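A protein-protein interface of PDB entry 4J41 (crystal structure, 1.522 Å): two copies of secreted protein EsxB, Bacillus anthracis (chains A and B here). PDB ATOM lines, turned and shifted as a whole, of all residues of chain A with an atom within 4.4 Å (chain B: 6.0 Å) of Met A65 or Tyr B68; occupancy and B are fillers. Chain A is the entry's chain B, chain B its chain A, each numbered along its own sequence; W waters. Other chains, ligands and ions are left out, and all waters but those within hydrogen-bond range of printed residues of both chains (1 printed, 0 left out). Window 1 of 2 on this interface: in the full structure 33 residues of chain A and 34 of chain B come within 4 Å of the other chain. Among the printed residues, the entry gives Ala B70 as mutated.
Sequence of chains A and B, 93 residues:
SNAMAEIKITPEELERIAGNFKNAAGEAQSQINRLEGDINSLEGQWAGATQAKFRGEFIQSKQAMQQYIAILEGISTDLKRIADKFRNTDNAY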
ATOM      1  N   ALA A  28     -28.290 -14.200 -12.762  1.00  0.00           N
ATOM      2  CA  ALA A  28     -27.042 -13.489 -12.970  1.00  0.00           C
ATOM      3  C   ALA A  28     -26.906 -12.347 -11.967  1.00  0.00           C
ATOM      4  O   ALA A  28     -25.836 -12.139 -11.386  1.00  0.00           O
ATOM      5  CB  ALA A  28     -26.998 -12.985 -14.394  1.00  0.00           C
ATOM      6  N   GLN A  31     -26.133 -13.829  -8.617  1.00  0.00           N
ATOM      7  CA  GLN A  31     -24.748 -14.276  -8.560  1.00  0.00           C
ATOM      8  C   GLN A  31     -23.791 -13.116  -8.292  1.00  0.00           C
ATOM      9  O   GLN A  31     -22.907 -13.214  -7.426  1.00  0.00           O
ATOM     10  CB  GLN A  31     -24.368 -15.003  -9.852  1.00  0.00           C
ATOM     11  CG  GLN A  31     -22.928 -15.501  -9.873  1.00  0.00           C
ATOM     12  CD  GLN A  31     -22.558 -16.133 -11.202  1.00  0.00           C
ATOM     13  OE1 GLN A  31     -21.965 -15.482 -12.061  1.00  0.00           O
ATOM     14  NE2 GLN A  31     -22.899 -17.404 -11.374  1.00  0.00           N
ATOM     15  N   ILE A  32     -23.974 -12.009  -8.999  1.00  0.00           N
ATOM     16  CA  ILE A  32     -23.094 -10.857  -8.835  1.00  0.00           C
ATOM     17  C   ILE A  32     -23.277 -10.263  -7.427  1.00  0.00           C
ATOM     18  O   ILE A  32     -22.306  -9.832  -6.798  1.00  0.00           O
ATOM     19  CB  ILE A  32     -23.292  -9.821 -10.004  1.00  0.00           C
ATOM     20  CG1 ILE A  32     -22.081  -8.901 -10.139  1.00  0.00           C
ATOM     21  CG2 ILE A  32     -24.542  -9.013  -9.818  1.00  0.00           C
ATOM     22  CD1 ILE A  32     -20.896  -9.595 -10.696  1.00  0.00           C
ATOM     23  N   LEU A  35     -21.271 -12.529  -4.970  1.00  0.00           N
ATOM     24  CA  LEU A  35     -19.831 -12.331  -5.102  1.00  0.00           C
ATOM     25  C   LEU A  35     -19.401 -10.971  -4.580  1.00  0.00           C
ATOM     26  O   LEU A  35     -18.316 -10.845  -4.012  1.00  0.00           O
ATOM     27  CB  LEU A  35     -19.381 -12.514  -6.550  1.00  0.00           C
ATOM     28  CG  LEU A  35     -19.576 -13.917  -7.130  1.00  0.00           C
ATOM     29  CD1 LEU A  35     -19.236 -13.920  -8.621  1.00  0.00           C
ATOM     30  CD2 LEU A  35     -18.742 -14.962  -6.385  1.00  0.00           C
ATOM     31  N   SER A  61     -16.067  -6.750 -13.512  1.00  0.00           N
ATOM     32  CA  SER A  61     -16.965  -7.882 -13.741  1.00  0.00           C
ATOM     33  C   SER A  61     -18.413  -7.430 -13.632  1.00  0.00           C
ATOM     34  O   SER A  61     -19.285  -7.892 -14.378  1.00  0.00           O
ATOM     35  CB  SER A  61     -16.668  -9.038 -12.775  1.00  0.00           C
ATOM     36  OG  SER A  61     -17.323  -8.882 -11.526  1.00  0.00           O
ATOM     37  N   LYS A  62     -18.659  -6.504 -12.715  1.00  0.00           N
ATOM     38  CA  LYS A  62     -19.999  -5.974 -12.471  1.00  0.00           C
ATOM     39  C   LYS A  62     -20.511  -5.171 -13.672  1.00  0.00           C
ATOM     40  O   LYS A  62     -21.688  -5.271 -14.043  1.00  0.00           O
ATOM     41  CB  LYS A  62     -19.990  -5.117 -11.206  1.00  0.00           C
ATOM     42  CG  LYS A  62     -21.350  -4.731 -10.680  1.00  0.00           C
ATOM     43  CD  LYS A  62     -21.196  -4.105  -9.305  1.00  0.00           C
ATOM     44  CE  LYS A  62     -22.532  -3.714  -8.711  1.00  0.00           C
ATOM     45  NZ  LYS A  62     -22.331  -3.061  -7.394  1.00  0.00           N
ATOM     46  N   GLN A  63     -19.625  -4.390 -14.287  1.00  0.00           N
ATOM     47  CA  GLN A  63     -19.956  -3.629 -15.487  1.00  0.00           C
ATOM     48  C   GLN A  63     -20.329  -4.568 -16.623  1.00  0.00           C
ATOM     49  O   GLN A  63     -21.310  -4.329 -17.345  1.00  0.00           O
ATOM     50  CB  GLN A  63     -18.776  -2.749 -15.905  1.00  0.00           C
ATOM     51  CG  GLN A  63     -18.468  -1.627 -14.926  1.00  0.00           C
ATOM     52  CD  GLN A  63     -17.052  -1.097 -15.074  1.00  0.00           C
ATOM     53  OE1 GLN A  63     -16.244  -1.652 -15.821  1.00  0.00           O
ATOM     54  NE2 GLN A  63     -16.744  -0.022 -14.356  1.00  0.00           N
ATOM     55  N   ALA A  64     -19.558  -5.640 -16.778  1.00  0.00           N
ATOM     56  CA  ALA A  64     -19.874  -6.639 -17.801  1.00  0.00           C
ATOM     57  C   ALA A  64     -21.226  -7.273 -17.540  1.00  0.00           C
ATOM     58  O   ALA A  64     -21.998  -7.505 -18.472  1.00  0.00           O
ATOM     59  CB  ALA A  64     -18.799  -7.701 -17.871  1.00  0.00           C
ATOM     60  N   MET A  65     -21.515  -7.570 -16.278  1.00  0.00           N
ATOM     61  CA  MET A  65     -22.781  -8.206 -15.954  1.00  0.00           C
ATOM     62  C   MET A  65     -23.970  -7.262 -16.104  1.00  0.00           C
ATOM     63  O   MET A  65     -25.055  -7.689 -16.505  1.00  0.00           O
ATOM     64  CB  MET A  65     -22.729  -8.817 -14.550  1.00  0.00           C
ATOM     65  CG  MET A  65     -22.356 -10.292 -14.561  1.00  0.00           C
ATOM     66  SD  MET A  65     -23.562 -11.272 -15.484  1.00  0.00           S
ATOM     67  CE  MET A  65     -24.952 -10.485 -14.761  1.00  0.00           C
ATOM     68  N   GLN A  66     -23.770  -5.983 -15.801  1.00  0.00           N
ATOM     69  CA  GLN A  66     -24.814  -4.983 -16.027  1.00  0.00           C
ATOM     70  C   GLN A  66     -25.200  -4.948 -17.504  1.00  0.00           C
ATOM     71  O   GLN A  66     -26.394  -4.930 -17.842  1.00  0.00           O
ATOM     72  CB  GLN A  66     -24.373  -3.597 -15.541  1.00  0.00           C
ATOM     73  CG  GLN A  66     -24.388  -3.448 -14.024  1.00  0.00           C
ATOM     74  CD  GLN A  66     -23.746  -2.156 -13.529  1.00  0.00           C
ATOM     75  OE1 GLN A  66     -23.265  -1.335 -14.315  1.00  0.00           O
ATOM     76  NE2 GLN A  66     -23.736  -1.976 -12.213  1.00  0.00           N
ATOM     77  N   GLN A  67     -24.198  -4.962 -18.383  1.00  0.00           N
ATOM     78  CA  GLN A  67     -24.438  -5.019 -19.827  1.00  0.00           C
ATOM     79  C   GLN A  67     -25.196  -6.288 -20.217  1.00  0.00           C
ATOM     80  O   GLN A  67     -26.171  -6.244 -20.981  1.00  0.00           O
ATOM     81  CB  GLN A  67     -23.107  -4.988 -20.594  1.00  0.00           C
ATOM     82  CG  GLN A  67     -22.343  -3.681 -20.564  1.00  0.00           C
ATOM     83  CD  GLN A  67     -21.061  -3.760 -21.383  1.00  0.00           C
ATOM     84  OE1 GLN A  67     -20.800  -4.762 -22.055  1.00  0.00           O
ATOM     85  NE2 GLN A  67     -20.257  -2.706 -21.328  1.00  0.00           N
ATOM     86  N   TYR A  68     -24.724  -7.422 -19.713  1.00  0.00           N
ATOM     87  CA  TYR A  68     -25.321  -8.723 -20.002  1.00  0.00           C
ATOM     88  C   TYR A  68     -26.794  -8.765 -19.616  1.00  0.00           C
ATOM     89  O   TYR A  68     -27.652  -9.177 -20.410  1.00  0.00           O
ATOM     90  CB  TYR A  68     -24.554  -9.799 -19.231  1.00  0.00           C
ATOM     91  CG  TYR A  68     -25.056 -11.214 -19.372  1.00  0.00           C
ATOM     92  CD1 TYR A  68     -24.884 -11.924 -20.558  1.00  0.00           C
ATOM     93  CD2 TYR A  68     -25.648 -11.860 -18.297  1.00  0.00           C
ATOM     94  CE1 TYR A  68     -25.321 -13.239 -20.673  1.00  0.00           C
ATOM     95  CE2 TYR A  68     -26.083 -13.173 -18.393  1.00  0.00           C
ATOM     96  CZ  TYR A  68     -25.920 -13.854 -19.593  1.00  0.00           C
ATOM     97  OH  TYR A  68     -26.348 -15.161 -19.685  1.00  0.00           O
ATOM     98  N   ILE A  69     -27.091  -8.318 -18.402  1.00  0.00           N
ATOM     99  CA  ILE A  69     -28.457  -8.358 -17.882  1.00  0.00           C
ATOM    100  C   ILE A  69     -29.384  -7.485 -18.719  1.00  0.00           C
ATOM    101  O   ILE A  69     -30.514  -7.878 -19.039  1.00  0.00           O
ATOM    102  CB  ILE A  69     -28.492  -7.907 -16.409  1.00  0.00           C
ATOM    103  CG1 ILE A  69     -27.931  -9.011 -15.528  1.00  0.00           C
ATOM    104  CG2 ILE A  69     -29.913  -7.576 -15.963  1.00  0.00           C
ATOM    105  CD1 ILE A  69     -27.735  -8.577 -14.072  1.00  0.00           C
ATOM    106  N   ALA B  24     -18.971 -19.814  -9.634  1.00  0.00           N
ATOM    107  CA  ALA B  24     -19.771 -18.821 -10.345  1.00  0.00           C
ATOM    108  C   ALA B  24     -19.403 -18.785 -11.821  1.00  0.00           C
ATOM    109  O   ALA B  24     -20.283 -18.676 -12.685  1.00  0.00           O
ATOM    110  CB  ALA B  24     -19.589 -17.444  -9.731  1.00  0.00           C
ATOM    111  N   ALA B  25     -18.110 -18.880 -12.113  1.00  0.00           N
ATOM    112  CA  ALA B  25     -17.638 -18.884 -13.500  1.00  0.00           C
ATOM    113  C   ALA B  25     -18.233 -20.063 -14.269  1.00  0.00           C
ATOM    114  O   ALA B  25     -18.655 -19.919 -15.428  1.00  0.00           O
ATOM    115  CB  ALA B  25     -16.110 -18.937 -13.532  1.00  0.00           C
ATOM    116  N   ALA B  28     -21.987 -19.551 -14.810  1.00  0.00           N
ATOM    117  CA  ALA B  28     -22.168 -18.531 -15.833  1.00  0.00           C
ATOM    118  C   ALA B  28     -21.968 -19.118 -17.230  1.00  0.00           C
ATOM    119  O   ALA B  28     -22.757 -18.847 -18.151  1.00  0.00           O
ATOM    120  CB  ALA B  28     -21.203 -17.366 -15.580  1.00  0.00           C
ATOM    121  N   GLN B  63     -20.461 -11.960 -25.543  1.00  0.00           N
ATOM    122  CA  GLN B  63     -19.159 -11.339 -25.367  1.00  0.00           C
ATOM    123  C   GLN B  63     -19.028 -10.723 -23.973  1.00  0.00           C
ATOM    124  O   GLN B  63     -17.965 -10.806 -23.351  1.00  0.00           O
ATOM    125  CB  GLN B  63     -18.886 -10.321 -26.477  1.00  0.00           C
ATOM    126  CG  GLN B  63     -18.602 -10.980 -27.818  1.00  0.00           C
ATOM    127  CD  GLN B  63     -17.390 -11.894 -27.772  1.00  0.00           C
ATOM    128  OE1 GLN B  63     -16.347 -11.532 -27.228  1.00  0.00           O
ATOM    129  NE2 GLN B  63     -17.525 -13.088 -28.336  1.00  0.00           N
ATOM    130  N   ALA B  64     -20.105 -10.122 -23.480  1.00  0.00           N
ATOM    131  CA  ALA B  64     -20.106  -9.603 -22.110  1.00  0.00           C
ATOM    132  C   ALA B  64     -19.855 -10.720 -21.112  1.00  0.00           C
ATOM    133  O   ALA B  64     -19.114 -10.543 -20.134  1.00  0.00           O
ATOM    134  CB  ALA B  64     -21.415  -8.901 -21.795  1.00  0.00           C
ATOM    135  N   MET B  65     -20.465 -11.875 -21.357  1.00  0.00           N
ATOM    136  CA  MET B  65     -20.316 -13.012 -20.463  1.00  0.00           C
ATOM    137  C   MET B  65     -18.904 -13.582 -20.517  1.00  0.00           C
ATOM    138  O   MET B  65     -18.351 -13.966 -19.479  1.00  0.00           O
ATOM    139  CB  MET B  65     -21.347 -14.092 -20.812  1.00  0.00           C
ATOM    140  CG  MET B  65     -21.350 -15.257 -19.860  1.00  0.00           C
ATOM    141  SD  MET B  65     -21.516 -14.738 -18.135  1.00  0.00           S
ATOM    142  CE  MET B  65     -23.236 -15.129 -17.832  1.00  0.00           C
ATOM    143  N   GLN B  66     -18.318 -13.633 -21.712  1.00  0.00           N
ATOM    144  CA  GLN B  66     -16.946 -14.112 -21.869  1.00  0.00           C
ATOM    145  C   GLN B  66     -15.997 -13.261 -21.042  1.00  0.00           C
ATOM    146  O   GLN B  66     -15.124 -13.789 -20.348  1.00  0.00           O
ATOM    147  CB  GLN B  66     -16.507 -14.113 -23.340  1.00  0.00           C
ATOM    148  CG  GLN B  66     -16.896 -15.380 -24.086  1.00  0.00           C
ATOM    149  CD  GLN B  66     -16.410 -15.409 -25.522  1.00  0.00           C
ATOM    150  OE1 GLN B  66     -15.390 -14.806 -25.864  1.00  0.00           O
ATOM    151  NE2 GLN B  66     -17.143 -16.117 -26.374  1.00  0.00           N
ATOM    152  N   GLN B  67     -16.177 -11.944 -21.112  1.00  0.00           N
ATOM    153  CA  GLN B  67     -15.372 -11.011 -20.326  1.00  0.00           C
ATOM    154  C   GLN B  67     -15.536 -11.261 -18.827  1.00  0.00           C
ATOM    155  O   GLN B  67     -14.550 -11.355 -18.090  1.00  0.00           O
ATOM    156  CB  GLN B  67     -15.754  -9.564 -20.669  1.00  0.00           C
ATOM    157  CG  GLN B  67     -15.369  -9.150 -22.086  1.00  0.00           C
ATOM    158  CD  GLN B  67     -16.029  -7.853 -22.537  1.00  0.00           C
ATOM    159  OE1 GLN B  67     -16.134  -7.585 -23.737  1.00  0.00           O
ATOM    160  NE2 GLN B  67     -16.473  -7.043 -21.581  1.00  0.00           N
ATOM    161  N   TYR B  68     -16.783 -11.378 -18.384  1.00  0.00           N
ATOM    162  CA  TYR B  68     -17.102 -11.640 -16.982  1.00  0.00           C
ATOM    163  C   TYR B  68     -16.453 -12.925 -16.479  1.00  0.00           C
ATOM    164  O   TYR B  68     -15.814 -12.940 -15.413  1.00  0.00           O
ATOM    165  CB  TYR B  68     -18.623 -11.741 -16.856  1.00  0.00           C
ATOM    166  CG  TYR B  68     -19.156 -12.113 -15.502  1.00  0.00           C
ATOM    167  CD1 TYR B  68     -19.141 -11.206 -14.449  1.00  0.00           C
ATOM    168  CD2 TYR B  68     -19.707 -13.359 -15.282  1.00  0.00           C
ATOM    169  CE1 TYR B  68     -19.649 -11.553 -13.209  1.00  0.00           C
ATOM    170  CE2 TYR B  68     -20.238 -13.716 -14.057  1.00  0.00           C
ATOM    171  CZ  TYR B  68     -20.200 -12.802 -13.017  1.00  0.00           C
ATOM    172  OH  TYR B  68     -20.722 -13.158 -11.799  1.00  0.00           O
ATOM    173  N   ILE B  69     -16.632 -14.009 -17.228  1.00  0.00           N
ATOM    174  CA  ILE B  69     -16.075 -15.302 -16.846  1.00  0.00           C
ATOM    175  C   ILE B  69     -14.555 -15.229 -16.692  1.00  0.00           C
ATOM    176  O   ILE B  69     -14.004 -15.738 -15.715  1.00  0.00           O
ATOM    177  CB  ILE B  69     -16.487 -16.405 -17.857  1.00  0.00           C
ATOM    178  CG1 ILE B  69     -17.988 -16.663 -17.754  1.00  0.00           C
ATOM    179  CG2 ILE B  69     -15.735 -17.693 -17.595  1.00  0.00           C
ATOM    180  CD1 ILE B  69     -18.528 -17.561 -18.861  1.00  0.00           C
ATOM    181  N   ALA B  70     -13.886 -14.572 -17.636  1.00  0.00           N
ATOM    182  CA  ALA B  70     -12.434 -14.422 -17.598  1.00  0.00           C
ATOM    183  C   ALA B  70     -11.997 -13.699 -16.332  1.00  0.00           C
ATOM    184  O   ALA B  70     -10.994 -14.062 -15.708  1.00  0.00           O
ATOM    185  CB  ALA B  70     -11.951 -13.667 -18.829  1.00  0.00           C
ATOM    186  N   ILE B  71     -12.750 -12.670 -15.958  1.00  0.00           N
ATOM    187  CA  ILE B  71     -12.439 -11.911 -14.748  1.00  0.00           C
ATOM    188  C   ILE B  71     -12.637 -12.769 -13.498  1.00  0.00           C
ATOM    189  O   ILE B  71     -11.779 -12.768 -12.594  1.00  0.00           O
ATOM    190  CB  ILE B  71     -13.278 -10.615 -14.654  1.00  0.00           C
ATOM    191  CG1 ILE B  71     -12.933  -9.673 -15.811  1.00  0.00           C
ATOM    192  CG2 ILE B  71     -13.066  -9.920 -13.302  1.00  0.00           C
ATOM    193  CD1 ILE B  71     -13.866  -8.488 -15.918  1.00  0.00           C
ATOM    194  N   LEU B  72     -13.746 -13.508 -13.436  1.00  0.00           N
ATOM    195  CA  LEU B  72     -14.006 -14.373 -12.280  1.00  0.00           C
ATOM    196  C   LEU B  72     -12.920 -15.430 -12.127  1.00  0.00           C
ATOM    197  O   LEU B  72     -12.467 -15.699 -11.021  1.00  0.00           O
ATOM    198  CB  LEU B  72     -15.373 -15.059 -12.386  1.00  0.00           C
ATOM    199  CG  LEU B  72     -16.634 -14.193 -12.381  1.00  0.00           C
ATOM    200  CD1 LEU B  72     -17.839 -15.054 -11.997  1.00  0.00           C
ATOM    201  CD2 LEU B  72     -16.512 -12.980 -11.475  1.00  0.00           C
ATOM    202  N   GLU B  73     -12.501 -16.038 -13.233  1.00  0.00           N
ATOM    203  CA  GLU B  73     -11.477 -17.068 -13.153  1.00  0.00           C
ATOM    204  C   GLU B  73     -10.144 -16.484 -12.692  1.00  0.00           C
ATOM    205  O   GLU B  73      -9.424 -17.120 -11.921  1.00  0.00           O
ATOM    206  CB  GLU B  73     -11.345 -17.818 -14.482  1.00  0.00           C
ATOM    207  CG  GLU B  73     -12.408 -18.893 -14.651  1.00  0.00           C
ATOM    208  CD  GLU B  73     -12.527 -19.386 -16.077  1.00  0.00           C
ATOM    209  OE1 GLU B  73     -11.926 -18.759 -16.975  1.00  0.00           O
ATOM    210  OE2 GLU B  73     -13.229 -20.396 -16.299  1.00  0.00           O
HETATM  211  O   HOH W   1     -17.626  -4.558 -20.081  1.00  0.00           O
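The side-chain amide oxygen (OE1) of Gln A31 is in hydrogen-bond range of the side-chain hydroxyl (OH) of Tyr B68 (2.6 Å). The side-chain amide nitrogen (NE2) of Gln A31 is in hydrogen-bond range of the backbone carbonyl oxygen (O) of Ala B24 (3.2 Å).
Among the printed residues, pairs that only touch across the chains: Met A65 with Tyr B68 (3.3 Å), Ser A61 with Tyr B68 (3.3 Å), Ile A32 with Tyr B68 (3.4 Å), Tyr A68 with Met B65 (3.5 Å), Leu A35 with Tyr B68 (3.6 Å), Ala A64 with Ala B64 (3.6 Å), Ser A61 with Ile B71 (3.7 Å), Leu A35 with Ala B24 (3.7 Å) and Leu A35 with Leu B72 (3.8 Å).
Printed residues of chain B within 4 Å of Leu A35: Ala B24, Tyr B68 and Leu B72. Of chain B, only Tyr B68 comes within 4 Å of Met A65. Gln A67 touches none of the printed residues of chain B. Printed residues of chain A within 4 Å of Ala B64: Ala A64. Of chain A, only Gln A31 (2.6 Å), Ile A32 (3.4 Å), Leu A35 (3.6 Å), Ser A61 (3.3 Å) and Met A65 (3.3 Å) come within 4 Å of Tyr B68. Of the printed residues of chain A, Leu B72 touches Leu A35. The nearest residue of chain A that does not touch Tyr B68 is Ala A64 (4.2 Å).
Hydrophobic or aromatic side chains of chain B that line the printed part of chain A: Ala B24, Ala B64, Met B65, Tyr B68, Ile B71 and Leu B72. Among the printed residues, 11 pairs touch across the chains. Among the printed residues, no Asp or Glu carboxylate lies within 4 Å of a Lys or Arg side-chain nitrogen of the other chain.
Ala A64 touches its own counterpart, Ala B64. Met A65 touches Tyr B68, and with the chains exchanged Tyr A68 touches Met B65. 8 positions are printed for both chains. Of the 11 pairs that touch across the chains among the printed residues, 3 have their exchanged pair printed and touching as well.
Water W1 bridges NE2 of Gln B67 (3.1 Å) and NE2 of Gln A67 (3.5 Å).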
